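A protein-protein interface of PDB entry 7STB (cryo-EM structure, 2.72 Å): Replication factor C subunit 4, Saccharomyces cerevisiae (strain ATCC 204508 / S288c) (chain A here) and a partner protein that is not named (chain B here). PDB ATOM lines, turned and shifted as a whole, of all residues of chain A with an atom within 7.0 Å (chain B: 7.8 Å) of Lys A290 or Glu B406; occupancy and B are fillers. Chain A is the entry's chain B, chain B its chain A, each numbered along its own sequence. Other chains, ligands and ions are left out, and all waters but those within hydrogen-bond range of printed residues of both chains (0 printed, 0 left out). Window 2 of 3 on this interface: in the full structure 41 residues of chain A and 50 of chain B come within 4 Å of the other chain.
OE2 of Glu B406 is in salt-bridge range of NZ of Lys A290.
O of Ile A289 sits close to OE1 of Glu B415.
The backbone NH (N) of Gly A293 is in hydrogen-bond range of the side-chain carboxylate (OE1) of Glu B415, at 2.8 Å.
Among the printed residues, pairs that only touch across the chains: Leu A286 with Glu B423, Met A297 with Asn B409, Leu A286 with Tyr B419, Lys A290 with Tyr B419, Ile A292 with Glu B415, Met A297 with Met B410 and His A296 with Glu B415.
OH of Tyr B419 lies close to SG of Cys B403, at 3.8 Å.
Arg A285 touches none of the printed residues of chain B.
Of the printed residues of chain B, Lys A290 touches Glu B406 and Tyr B419.
Glu A291 touches none of the printed residues of chain B.
Of the printed residues of chain B, His A296 touches Glu B415.
Glu B406 touches just one residue of chain A: Lys A290 (2.4 Å).
Of the printed residues of chain A, Asn B409 touches Met A297.
Of the printed residues of chain A, Glu B415 touches Ile A289 (2.9 Å), Ile A292 (3.5 Å), Gly A293 (2.8 Å) and His A296 (3.8 Å).
Printed residues of chain A within 4 Å of Glu B423: Leu A286.
The nearest residue of chain B that does not touch Lys A290 is Met B410 (4.4 Å).
The nearest residue of chain A that does not touch Glu B406 is Leu A294 (4.6 Å).
The nearest printed residue of chain A that does not touch Glu B415 is Lys A290 (5.0 Å).
Of the 16 printed residues of chain A, 7 touch a printed residue of chain B.
Hydrophobic or aromatic side chains of chain A that line the printed part of chain B: Leu A286, Ile A289, Ile A292, His A296 and Met A297.
Printed residues of chain B that touch a printed residue of chain A: Glu B406, Asn B409, Met B410, Glu B415, Tyr B419 and Glu B423.
Hydrophobic or aromatic side chains of chain B that line the printed part of chain A: Met B410 and Tyr B419.
Among the printed residues, 10 pairs touch across the chains.
Among the printed residues, Asp or Glu carboxylates within 4 Å of a Lys or Arg side-chain nitrogen of the other chain: Lys A290 with Glu B406 (2.4 Å).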
ATOM      1  N   VAL A 284     -18.603 -24.980   6.585  1.00  0.00           N
ATOM      2  CA  VAL A 284     -19.669 -24.025   6.289  1.00  0.00           C
ATOM      3  C   VAL A 284     -20.706 -24.031   7.406  1.00  0.00           C
ATOM      4  O   VAL A 284     -21.113 -22.975   7.907  1.00  0.00           O
ATOM      5  CB  VAL A 284     -20.308 -24.341   4.926  1.00  0.00           C
ATOM      6  CG1 VAL A 284     -21.331 -23.276   4.559  1.00  0.00           C
ATOM      7  CG2 VAL A 284     -19.239 -24.454   3.848  1.00  0.00           C
ATOM      8  N   ARG A 285     -21.146 -25.224   7.814  1.00  0.00           N
ATOM      9  CA  ARG A 285     -22.114 -25.324   8.900  1.00  0.00           C
ATOM     10  C   ARG A 285     -21.556 -24.723  10.181  1.00  0.00           C
ATOM     11  O   ARG A 285     -22.281 -24.072  10.944  1.00  0.00           O
ATOM     12  CB  ARG A 285     -22.498 -26.788   9.115  1.00  0.00           C
ATOM     13  CG  ARG A 285     -23.598 -27.012  10.142  1.00  0.00           C
ATOM     14  CD  ARG A 285     -23.415 -28.340  10.854  1.00  0.00           C
ATOM     15  NE  ARG A 285     -23.110 -29.420   9.921  1.00  0.00           N
ATOM     16  CZ  ARG A 285     -23.958 -30.372   9.554  1.00  0.00           C
ATOM     17  NH1 ARG A 285     -25.196 -30.421  10.020  1.00  0.00           N
ATOM     18  NH2 ARG A 285     -23.553 -31.302   8.693  1.00  0.00           N
ATOM     19  N   LEU A 286     -20.266 -24.935  10.433  1.00  0.00           N
ATOM     20  CA  LEU A 286     -19.635 -24.392  11.629  1.00  0.00           C
ATOM     21  C   LEU A 286     -19.664 -22.868  11.618  1.00  0.00           C
ATOM     22  O   LEU A 286     -19.986 -22.230  12.627  1.00  0.00           O
ATOM     23  CB  LEU A 286     -18.201 -24.908  11.715  1.00  0.00           C
ATOM     24  CG  LEU A 286     -17.402 -24.497  12.942  1.00  0.00           C
ATOM     25  CD1 LEU A 286     -18.067 -25.055  14.175  1.00  0.00           C
ATOM     26  CD2 LEU A 286     -15.978 -24.994  12.821  1.00  0.00           C
ATOM     27  N   GLU A 287     -19.328 -22.267  10.476  1.00  0.00           N
ATOM     28  CA  GLU A 287     -19.356 -20.811  10.379  1.00  0.00           C
ATOM     29  C   GLU A 287     -20.777 -20.277  10.527  1.00  0.00           C
ATOM     30  O   GLU A 287     -20.993 -19.233  11.156  1.00  0.00           O
ATOM     31  CB  GLU A 287     -18.743 -20.361   9.055  1.00  0.00           C
ATOM     32  CG  GLU A 287     -17.278 -20.736   8.890  1.00  0.00           C
ATOM     33  CD  GLU A 287     -16.362 -19.914   9.775  1.00  0.00           C
ATOM     34  OE1 GLU A 287     -16.675 -18.731  10.023  1.00  0.00           O
ATOM     35  OE2 GLU A 287     -15.329 -20.452  10.225  1.00  0.00           O
ATOM     36  N   MET A 288     -21.759 -20.975   9.949  1.00  0.00           N
ATOM     37  CA  MET A 288     -23.150 -20.570  10.133  1.00  0.00           C
ATOM     38  C   MET A 288     -23.544 -20.607  11.604  1.00  0.00           C
ATOM     39  O   MET A 288     -24.209 -19.690  12.098  1.00  0.00           O
ATOM     40  CB  MET A 288     -24.077 -21.467   9.310  1.00  0.00           C
ATOM     41  CG  MET A 288     -23.790 -21.474   7.818  1.00  0.00           C
ATOM     42  SD  MET A 288     -24.789 -22.669   6.908  1.00  0.00           S
ATOM     43  CE  MET A 288     -26.448 -22.105   7.272  1.00  0.00           C
ATOM     44  N   ILE A 289     -23.145 -21.660  12.319  1.00  0.00           N
ATOM     45  CA  ILE A 289     -23.449 -21.744  13.746  1.00  0.00           C
ATOM     46  C   ILE A 289     -22.784 -20.597  14.496  1.00  0.00           C
ATOM     47  O   ILE A 289     -23.366 -20.019  15.423  1.00  0.00           O
ATOM     48  CB  ILE A 289     -23.016 -23.112  14.305  1.00  0.00           C
ATOM     49  CG1 ILE A 289     -23.918 -24.219  13.755  1.00  0.00           C
ATOM     50  CG2 ILE A 289     -23.055 -23.101  15.826  1.00  0.00           C
ATOM     51  CD1 ILE A 289     -23.340 -25.611  13.902  1.00  0.00           C
ATOM     52  N   LYS A 290     -21.554 -20.255  14.114  1.00  0.00           N
ATOM     53  CA  LYS A 290     -20.851 -19.149  14.757  1.00  0.00           C
ATOM     54  C   LYS A 290     -21.607 -17.836  14.580  1.00  0.00           C
ATOM     55  O   LYS A 290     -21.819 -17.084  15.543  1.00  0.00           O
ATOM     56  CB  LYS A 290     -19.442 -19.045  14.174  1.00  0.00           C
ATOM     57  CG  LYS A 290     -18.561 -17.988  14.802  1.00  0.00           C
ATOM     58  CD  LYS A 290     -17.184 -18.011  14.166  1.00  0.00           C
ATOM     59  CE  LYS A 290     -16.243 -17.036  14.833  1.00  0.00           C
ATOM     60  NZ  LYS A 290     -16.638 -15.622  14.588  1.00  0.00           N
ATOM     61  N   GLU A 291     -22.018 -17.537  13.345  1.00  0.00           N
ATOM     62  CA  GLU A 291     -22.755 -16.301  13.097  1.00  0.00           C
ATOM     63  C   GLU A 291     -24.093 -16.305  13.828  1.00  0.00           C
ATOM     64  O   GLU A 291     -24.525 -15.272  14.359  1.00  0.00           O
ATOM     65  CB  GLU A 291     -22.968 -16.100  11.595  1.00  0.00           C
ATOM     66  CG  GLU A 291     -21.708 -16.125  10.718  1.00  0.00           C
ATOM     67  CD  GLU A 291     -20.551 -15.267  11.223  1.00  0.00           C
ATOM     68  OE1 GLU A 291     -19.510 -15.225  10.534  1.00  0.00           O
ATOM     69  OE2 GLU A 291     -20.676 -14.611  12.276  1.00  0.00           O
ATOM     70  N   ILE A 292     -24.766 -17.455  13.860  1.00  0.00           N
ATOM     71  CA  ILE A 292     -26.036 -17.552  14.571  1.00  0.00           C
ATOM     72  C   ILE A 292     -25.835 -17.268  16.052  1.00  0.00           C
ATOM     73  O   ILE A 292     -26.654 -16.594  16.687  1.00  0.00           O
ATOM     74  CB  ILE A 292     -26.673 -18.934  14.335  1.00  0.00           C
ATOM     75  CG1 ILE A 292     -27.192 -19.032  12.899  1.00  0.00           C
ATOM     76  CG2 ILE A 292     -27.795 -19.181  15.333  1.00  0.00           C
ATOM     77  CD1 ILE A 292     -27.537 -20.438  12.463  1.00  0.00           C
ATOM     78  N   GLY A 293     -24.747 -17.781  16.630  1.00  0.00           N
ATOM     79  CA  GLY A 293     -24.471 -17.509  18.031  1.00  0.00           C
ATOM     80  C   GLY A 293     -24.184 -16.046  18.296  1.00  0.00           C
ATOM     81  O   GLY A 293     -24.635 -15.486  19.299  1.00  0.00           O
ATOM     82  N   LEU A 294     -23.422 -15.406  17.409  1.00  0.00           N
ATOM     83  CA  LEU A 294     -23.169 -13.978  17.577  1.00  0.00           C
ATOM     84  C   LEU A 294     -24.471 -13.185  17.525  1.00  0.00           C
ATOM     85  O   LEU A 294     -24.690 -12.272  18.335  1.00  0.00           O
ATOM     86  CB  LEU A 294     -22.192 -13.488  16.509  1.00  0.00           C
ATOM     87  CG  LEU A 294     -20.775 -14.060  16.596  1.00  0.00           C
ATOM     88  CD1 LEU A 294     -19.948 -13.607  15.405  1.00  0.00           C
ATOM     89  CD2 LEU A 294     -20.098 -13.662  17.898  1.00  0.00           C
ATOM     90  N   THR A 295     -25.354 -13.526  16.585  1.00  0.00           N
ATOM     91  CA  THR A 295     -26.640 -12.840  16.498  1.00  0.00           C
ATOM     92  C   THR A 295     -27.492 -13.097  17.738  1.00  0.00           C
ATOM     93  O   THR A 295     -28.171 -12.189  18.231  1.00  0.00           O
ATOM     94  CB  THR A 295     -27.381 -13.276  15.235  1.00  0.00           C
ATOM     95  OG1 THR A 295     -26.595 -12.945  14.086  1.00  0.00           O
ATOM     96  CG2 THR A 295     -28.734 -12.585  15.138  1.00  0.00           C
ATOM     97  N   HIS A 296     -27.478 -14.329  18.248  1.00  0.00           N
ATOM     98  CA  HIS A 296     -28.227 -14.637  19.462  1.00  0.00           C
ATOM     99  C   HIS A 296     -27.720 -13.811  20.636  1.00  0.00           C
ATOM    100  O   HIS A 296     -28.514 -13.294  21.433  1.00  0.00           O
ATOM    101  CB  HIS A 296     -28.126 -16.132  19.768  1.00  0.00           C
ATOM    102  CG  HIS A 296     -29.018 -16.585  20.881  1.00  0.00           C
ATOM    103  ND1 HIS A 296     -28.942 -17.848  21.426  1.00  0.00           N
ATOM    104  CD2 HIS A 296     -30.007 -15.947  21.550  1.00  0.00           C
ATOM    105  CE1 HIS A 296     -29.844 -17.968  22.383  1.00  0.00           C
ATOM    106  NE2 HIS A 296     -30.503 -16.828  22.478  1.00  0.00           N
ATOM    107  N   MET A 297     -26.398 -13.681  20.763  1.00  0.00           N
ATOM    108  CA  MET A 297     -25.836 -12.803  21.785  1.00  0.00           C
ATOM    109  C   MET A 297     -26.350 -11.380  21.621  1.00  0.00           C
ATOM    110  O   MET A 297     -26.850 -10.773  22.574  1.00  0.00           O
ATOM    111  CB  MET A 297     -24.311 -12.811  21.712  1.00  0.00           C
ATOM    112  CG  MET A 297     -23.654 -14.120  22.078  1.00  0.00           C
ATOM    113  SD  MET A 297     -21.869 -14.003  21.862  1.00  0.00           S
ATOM    114  CE  MET A 297     -21.436 -12.904  23.209  1.00  0.00           C
ATOM    115  N   LYS A 315     -24.049 -12.605   6.563  1.00  0.00           N
ATOM    116  CA  LYS A 315     -22.829 -13.311   6.938  1.00  0.00           C
ATOM    117  C   LYS A 315     -22.898 -14.777   6.530  1.00  0.00           C
ATOM    118  O   LYS A 315     -21.914 -15.339   6.033  1.00  0.00           O
ATOM    119  CB  LYS A 315     -22.586 -13.184   8.442  1.00  0.00           C
ATOM    120  CG  LYS A 315     -22.178 -11.789   8.886  1.00  0.00           C
ATOM    121  CD  LYS A 315     -21.764 -11.766  10.348  1.00  0.00           C
ATOM    122  CE  LYS A 315     -22.958 -11.955  11.269  1.00  0.00           C
ATOM    123  NZ  LYS A 315     -22.595 -11.775  12.701  1.00  0.00           N
ATOM    124  N   LEU A 319     -20.427 -16.658   3.905  1.00  0.00           N
ATOM    125  CA  LEU A 319     -19.726 -17.890   4.249  1.00  0.00           C
ATOM    126  C   LEU A 319     -19.984 -18.978   3.216  1.00  0.00           C
ATOM    127  O   LEU A 319     -19.069 -19.726   2.850  1.00  0.00           O
ATOM    128  CB  LEU A 319     -20.153 -18.357   5.639  1.00  0.00           C
ATOM    129  CG  LEU A 319     -19.729 -17.429   6.778  1.00  0.00           C
ATOM    130  CD1 LEU A 319     -20.558 -17.704   8.023  1.00  0.00           C
ATOM    131  CD2 LEU A 319     -18.239 -17.574   7.059  1.00  0.00           C
ATOM    132  N   LYS B 377     -13.737 -27.283  28.195  1.00  0.00           N
ATOM    133  CA  LYS B 377     -13.021 -26.373  27.309  1.00  0.00           C
ATOM    134  C   LYS B 377     -11.562 -26.240  27.731  1.00  0.00           C
ATOM    135  O   LYS B 377     -10.655 -26.246  26.888  1.00  0.00           O
ATOM    136  CB  LYS B 377     -13.713 -25.009  27.312  1.00  0.00           C
ATOM    137  CG  LYS B 377     -13.220 -24.033  26.255  1.00  0.00           C
ATOM    138  CD  LYS B 377     -13.509 -24.504  24.833  1.00  0.00           C
ATOM    139  CE  LYS B 377     -15.001 -24.617  24.546  1.00  0.00           C
ATOM    140  NZ  LYS B 377     -15.685 -23.297  24.610  1.00  0.00           N
ATOM    141  N   SER B 399      -5.154 -21.651  15.232  1.00  0.00           N
ATOM    142  CA  SER B 399      -6.573 -21.600  14.900  1.00  0.00           C
ATOM    143  C   SER B 399      -7.421 -22.176  16.027  1.00  0.00           C
ATOM    144  O   SER B 399      -8.452 -21.602  16.396  1.00  0.00           O
ATOM    145  CB  SER B 399      -6.832 -22.353  13.595  1.00  0.00           C
ATOM    146  OG  SER B 399      -6.390 -21.600  12.480  1.00  0.00           O
ATOM    147  N   ILE B 400      -6.995 -23.307  16.593  1.00  0.00           N
ATOM    148  CA  ILE B 400      -7.755 -23.923  17.678  1.00  0.00           C
ATOM    149  C   ILE B 400      -7.829 -22.981  18.873  1.00  0.00           C
ATOM    150  O   ILE B 400      -8.899 -22.774  19.460  1.00  0.00           O
ATOM    151  CB  ILE B 400      -7.130 -25.275  18.068  1.00  0.00           C
ATOM    152  CG1 ILE B 400      -7.337 -26.300  16.951  1.00  0.00           C
ATOM    153  CG2 ILE B 400      -7.729 -25.777  19.377  1.00  0.00           C
ATOM    154  CD1 ILE B 400      -6.458 -27.526  17.077  1.00  0.00           C
ATOM    155  N   VAL B 401      -6.692 -22.395  19.253  1.00  0.00           N
ATOM    156  CA  VAL B 401      -6.672 -21.536  20.432  1.00  0.00           C
ATOM    157  C   VAL B 401      -7.482 -20.269  20.184  1.00  0.00           C
ATOM    158  O   VAL B 401      -8.175 -19.778  21.083  1.00  0.00           O
ATOM    159  CB  VAL B 401      -5.222 -21.214  20.841  1.00  0.00           C
ATOM    160  CG1 VAL B 401      -5.210 -20.316  22.066  1.00  0.00           C
ATOM    161  CG2 VAL B 401      -4.453 -22.493  21.130  1.00  0.00           C
ATOM    162  N   ASP B 402      -7.410 -19.716  18.972  1.00  0.00           N
ATOM    163  CA  ASP B 402      -8.212 -18.542  18.645  1.00  0.00           C
ATOM    164  C   ASP B 402      -9.698 -18.859  18.728  1.00  0.00           C
ATOM    165  O   ASP B 402     -10.487 -18.063  19.253  1.00  0.00           O
ATOM    166  CB  ASP B 402      -7.844 -18.040  17.249  1.00  0.00           C
ATOM    167  CG  ASP B 402      -8.594 -16.781  16.863  1.00  0.00           C
ATOM    168  OD1 ASP B 402      -9.208 -16.155  17.749  1.00  0.00           O
ATOM    169  OD2 ASP B 402      -8.567 -16.418  15.668  1.00  0.00           O
ATOM    170  N   CYS B 403     -10.099 -20.025  18.217  1.00  0.00           N
ATOM    171  CA  CYS B 403     -11.500 -20.418  18.294  1.00  0.00           C
ATOM    172  C   CYS B 403     -11.949 -20.578  19.741  1.00  0.00           C
ATOM    173  O   CYS B 403     -13.042 -20.135  20.111  1.00  0.00           O
ATOM    174  CB  CYS B 403     -11.718 -21.716  17.521  1.00  0.00           C
ATOM    175  SG  CYS B 403     -13.305 -22.489  17.843  1.00  0.00           S
ATOM    176  N   LEU B 404     -11.121 -21.210  20.577  1.00  0.00           N
ATOM    177  CA  LEU B 404     -11.484 -21.365  21.985  1.00  0.00           C
ATOM    178  C   LEU B 404     -11.587 -20.009  22.676  1.00  0.00           C
ATOM    179  O   LEU B 404     -12.504 -19.775  23.475  1.00  0.00           O
ATOM    180  CB  LEU B 404     -10.464 -22.254  22.698  1.00  0.00           C
ATOM    181  CG  LEU B 404     -10.258 -23.686  22.184  1.00  0.00           C
ATOM    182  CD1 LEU B 404      -9.218 -24.393  23.037  1.00  0.00           C
ATOM    183  CD2 LEU B 404     -11.545 -24.499  22.153  1.00  0.00           C
ATOM    184  N   SER B 405     -10.658 -19.100  22.377  1.00  0.00           N
ATOM    185  CA  SER B 405     -10.704 -17.772  22.972  1.00  0.00           C
ATOM    186  C   SER B 405     -11.977 -17.039  22.576  1.00  0.00           C
ATOM    187  O   SER B 405     -12.611 -16.383  23.411  1.00  0.00           O
ATOM    188  CB  SER B 405      -9.472 -16.968  22.553  1.00  0.00           C
ATOM    189  OG  SER B 405      -9.458 -15.696  23.174  1.00  0.00           O
ATOM    190  N   GLU B 406     -12.368 -17.134  21.305  1.00  0.00           N
ATOM    191  CA  GLU B 406     -13.576 -16.443  20.866  1.00  0.00           C
ATOM    192  C   GLU B 406     -14.825 -17.097  21.449  1.00  0.00           C
ATOM    193  O   GLU B 406     -15.817 -16.415  21.728  1.00  0.00           O
ATOM    194  CB  GLU B 406     -13.635 -16.404  19.341  1.00  0.00           C
ATOM    195  CG  GLU B 406     -14.819 -15.628  18.798  1.00  0.00           C
ATOM    196  CD  GLU B 406     -14.824 -15.556  17.288  1.00  0.00           C
ATOM    197  OE1 GLU B 406     -13.912 -16.133  16.661  1.00  0.00           O
ATOM    198  OE2 GLU B 406     -15.737 -14.915  16.727  1.00  0.00           O
ATOM    199  N   CYS B 407     -14.797 -18.418  21.636  1.00  0.00           N
ATOM    200  CA  CYS B 407     -15.887 -19.084  22.342  1.00  0.00           C
ATOM    201  C   CYS B 407     -16.000 -18.591  23.776  1.00  0.00           C
ATOM    202  O   CYS B 407     -17.109 -18.485  24.313  1.00  0.00           O
ATOM    203  CB  CYS B 407     -15.682 -20.599  22.330  1.00  0.00           C
ATOM    204  SG  CYS B 407     -15.989 -21.391  20.741  1.00  0.00           S
ATOM    205  N   ASP B 408     -14.866 -18.293  24.413  1.00  0.00           N
ATOM    206  CA  ASP B 408     -14.892 -17.818  25.792  1.00  0.00           C
ATOM    207  C   ASP B 408     -15.693 -16.528  25.947  1.00  0.00           C
ATOM    208  O   ASP B 408     -16.128 -16.215  27.060  1.00  0.00           O
ATOM    209  CB  ASP B 408     -13.467 -17.604  26.300  1.00  0.00           C
ATOM    210  CG  ASP B 408     -13.419 -17.276  27.780  1.00  0.00           C
ATOM    211  OD1 ASP B 408     -14.069 -17.990  28.571  1.00  0.00           O
ATOM    212  OD2 ASP B 408     -12.731 -16.302  28.151  1.00  0.00           O
ATOM    213  N   ASN B 409     -15.895 -15.777  24.868  1.00  0.00           N
ATOM    214  CA  ASN B 409     -16.623 -14.515  24.917  1.00  0.00           C
ATOM    215  C   ASN B 409     -18.119 -14.664  24.675  1.00  0.00           C
ATOM    216  O   ASN B 409     -18.828 -13.653  24.666  1.00  0.00           O
ATOM    217  CB  ASN B 409     -16.060 -13.537  23.883  1.00  0.00           C
ATOM    218  CG  ASN B 409     -14.936 -12.691  24.430  1.00  0.00           C
ATOM    219  OD1 ASN B 409     -14.338 -13.015  25.454  1.00  0.00           O
ATOM    220  ND2 ASN B 409     -14.659 -11.584  23.757  1.00  0.00           N
ATOM    221  N   MET B 410     -18.623 -15.882  24.486  1.00  0.00           N
ATOM    222  CA  MET B 410     -20.021 -16.092  24.139  1.00  0.00           C
ATOM    223  C   MET B 410     -20.889 -16.386  25.357  1.00  0.00           C
ATOM    224  O   MET B 410     -21.982 -16.943  25.212  1.00  0.00           O
ATOM    225  CB  MET B 410     -20.144 -17.211  23.106  1.00  0.00           C
ATOM    226  CG  MET B 410     -19.548 -16.845  21.753  1.00  0.00           C
ATOM    227  SD  MET B 410     -19.677 -18.155  20.524  1.00  0.00           S
ATOM    228  CE  MET B 410     -18.807 -17.413  19.147  1.00  0.00           C
ATOM    229  N   ASN B 411     -20.425 -16.021  26.553  1.00  0.00           N
ATOM    230  CA  ASN B 411     -21.227 -16.121  27.771  1.00  0.00           C
ATOM    231  C   ASN B 411     -21.747 -17.541  27.980  1.00  0.00           C
ATOM    232  O   ASN B 411     -22.851 -17.752  28.487  1.00  0.00           O
ATOM    233  CB  ASN B 411     -22.382 -15.119  27.747  1.00  0.00           C
ATOM    234  CG  ASN B 411     -21.911 -13.685  27.882  1.00  0.00           C
ATOM    235  OD1 ASN B 411     -21.023 -13.384  28.680  1.00  0.00           O
ATOM    236  ND2 ASN B 411     -22.502 -12.790  27.099  1.00  0.00           N
ATOM    237  N   GLU B 415     -24.242 -23.210  21.888  1.00  0.00           N
ATOM    238  CA  GLU B 415     -23.726 -23.217  20.529  1.00  0.00           C
ATOM    239  C   GLU B 415     -22.312 -22.662  20.442  1.00  0.00           C
ATOM    240  O   GLU B 415     -21.602 -22.973  19.483  1.00  0.00           O
ATOM    241  CB  GLU B 415     -24.679 -22.450  19.612  1.00  0.00           C
ATOM    242  CG  GLU B 415     -24.755 -20.964  19.842  1.00  0.00           C
ATOM    243  CD  GLU B 415     -25.574 -20.286  18.768  1.00  0.00           C
ATOM    244  OE1 GLU B 415     -25.197 -20.382  17.583  1.00  0.00           O
ATOM    245  OE2 GLU B 415     -26.601 -19.661  19.108  1.00  0.00           O
ATOM    246  N   SER B 416     -21.869 -21.884  21.431  1.00  0.00           N
ATOM    247  CA  SER B 416     -20.448 -21.563  21.520  1.00  0.00           C
ATOM    248  C   SER B 416     -19.625 -22.826  21.740  1.00  0.00           C
ATOM    249  O   SER B 416     -18.584 -23.026  21.097  1.00  0.00           O
ATOM    250  CB  SER B 416     -20.205 -20.564  22.650  1.00  0.00           C
ATOM    251  OG  SER B 416     -20.212 -21.209  23.911  1.00  0.00           O
ATOM    252  N   GLU B 418     -20.627 -25.818  20.896  1.00  0.00           N
ATOM    253  CA  GLU B 418     -20.737 -26.527  19.626  1.00  0.00           C
ATOM    254  C   GLU B 418     -19.679 -26.038  18.643  1.00  0.00           C
ATOM    255  O   GLU B 418     -18.973 -26.838  18.021  1.00  0.00           O
ATOM    256  CB  GLU B 418     -22.137 -26.344  19.042  1.00  0.00           C
ATOM    257  CG  GLU B 418     -23.257 -26.937  19.896  1.00  0.00           C
ATOM    258  CD  GLU B 418     -23.822 -28.232  19.340  1.00  0.00           C
ATOM    259  OE1 GLU B 418     -23.465 -28.617  18.206  1.00  0.00           O
ATOM    260  OE2 GLU B 418     -24.635 -28.868  20.042  1.00  0.00           O
ATOM    261  N   TYR B 419     -19.558 -24.718  18.498  1.00  0.00           N
ATOM    262  CA  TYR B 419     -18.580 -24.150  17.578  1.00  0.00           C
ATOM    263  C   TYR B 419     -17.167 -24.573  17.952  1.00  0.00           C
ATOM    264  O   TYR B 419     -16.383 -24.988  17.090  1.00  0.00           O
ATOM    265  CB  TYR B 419     -18.706 -22.626  17.566  1.00  0.00           C
ATOM    266  CG  TYR B 419     -17.527 -21.907  16.949  1.00  0.00           C
ATOM    267  CD1 TYR B 419     -17.057 -22.251  15.690  1.00  0.00           C
ATOM    268  CD2 TYR B 419     -16.883 -20.883  17.627  1.00  0.00           C
ATOM    269  CE1 TYR B 419     -15.981 -21.597  15.126  1.00  0.00           C
ATOM    270  CE2 TYR B 419     -15.806 -20.225  17.071  1.00  0.00           C
ATOM    271  CZ  TYR B 419     -15.359 -20.586  15.821  1.00  0.00           C
ATOM    272  OH  TYR B 419     -14.286 -19.933  15.260  1.00  0.00           O
ATOM    273  N   GLU B 423     -14.923 -26.972  15.564  1.00  0.00           N
ATOM    274  CA  GLU B 423     -13.681 -26.447  15.007  1.00  0.00           C
ATOM    275  C   GLU B 423     -12.509 -27.360  15.336  1.00  0.00           C
ATOM    276  O   GLU B 423     -11.683 -27.667  14.469  1.00  0.00           O
ATOM    277  CB  GLU B 423     -13.421 -25.037  15.538  1.00  0.00           C
ATOM    278  CG  GLU B 423     -12.159 -24.377  14.985  1.00  0.00           C
ATOM    279  CD  GLU B 423     -12.222 -24.117  13.494  1.00  0.00           C
ATOM    280  OE1 GLU B 423     -13.339 -23.973  12.958  1.00  0.00           O
ATOM    281  OE2 GLU B 423     -11.151 -24.058  12.854  1.00  0.00           O
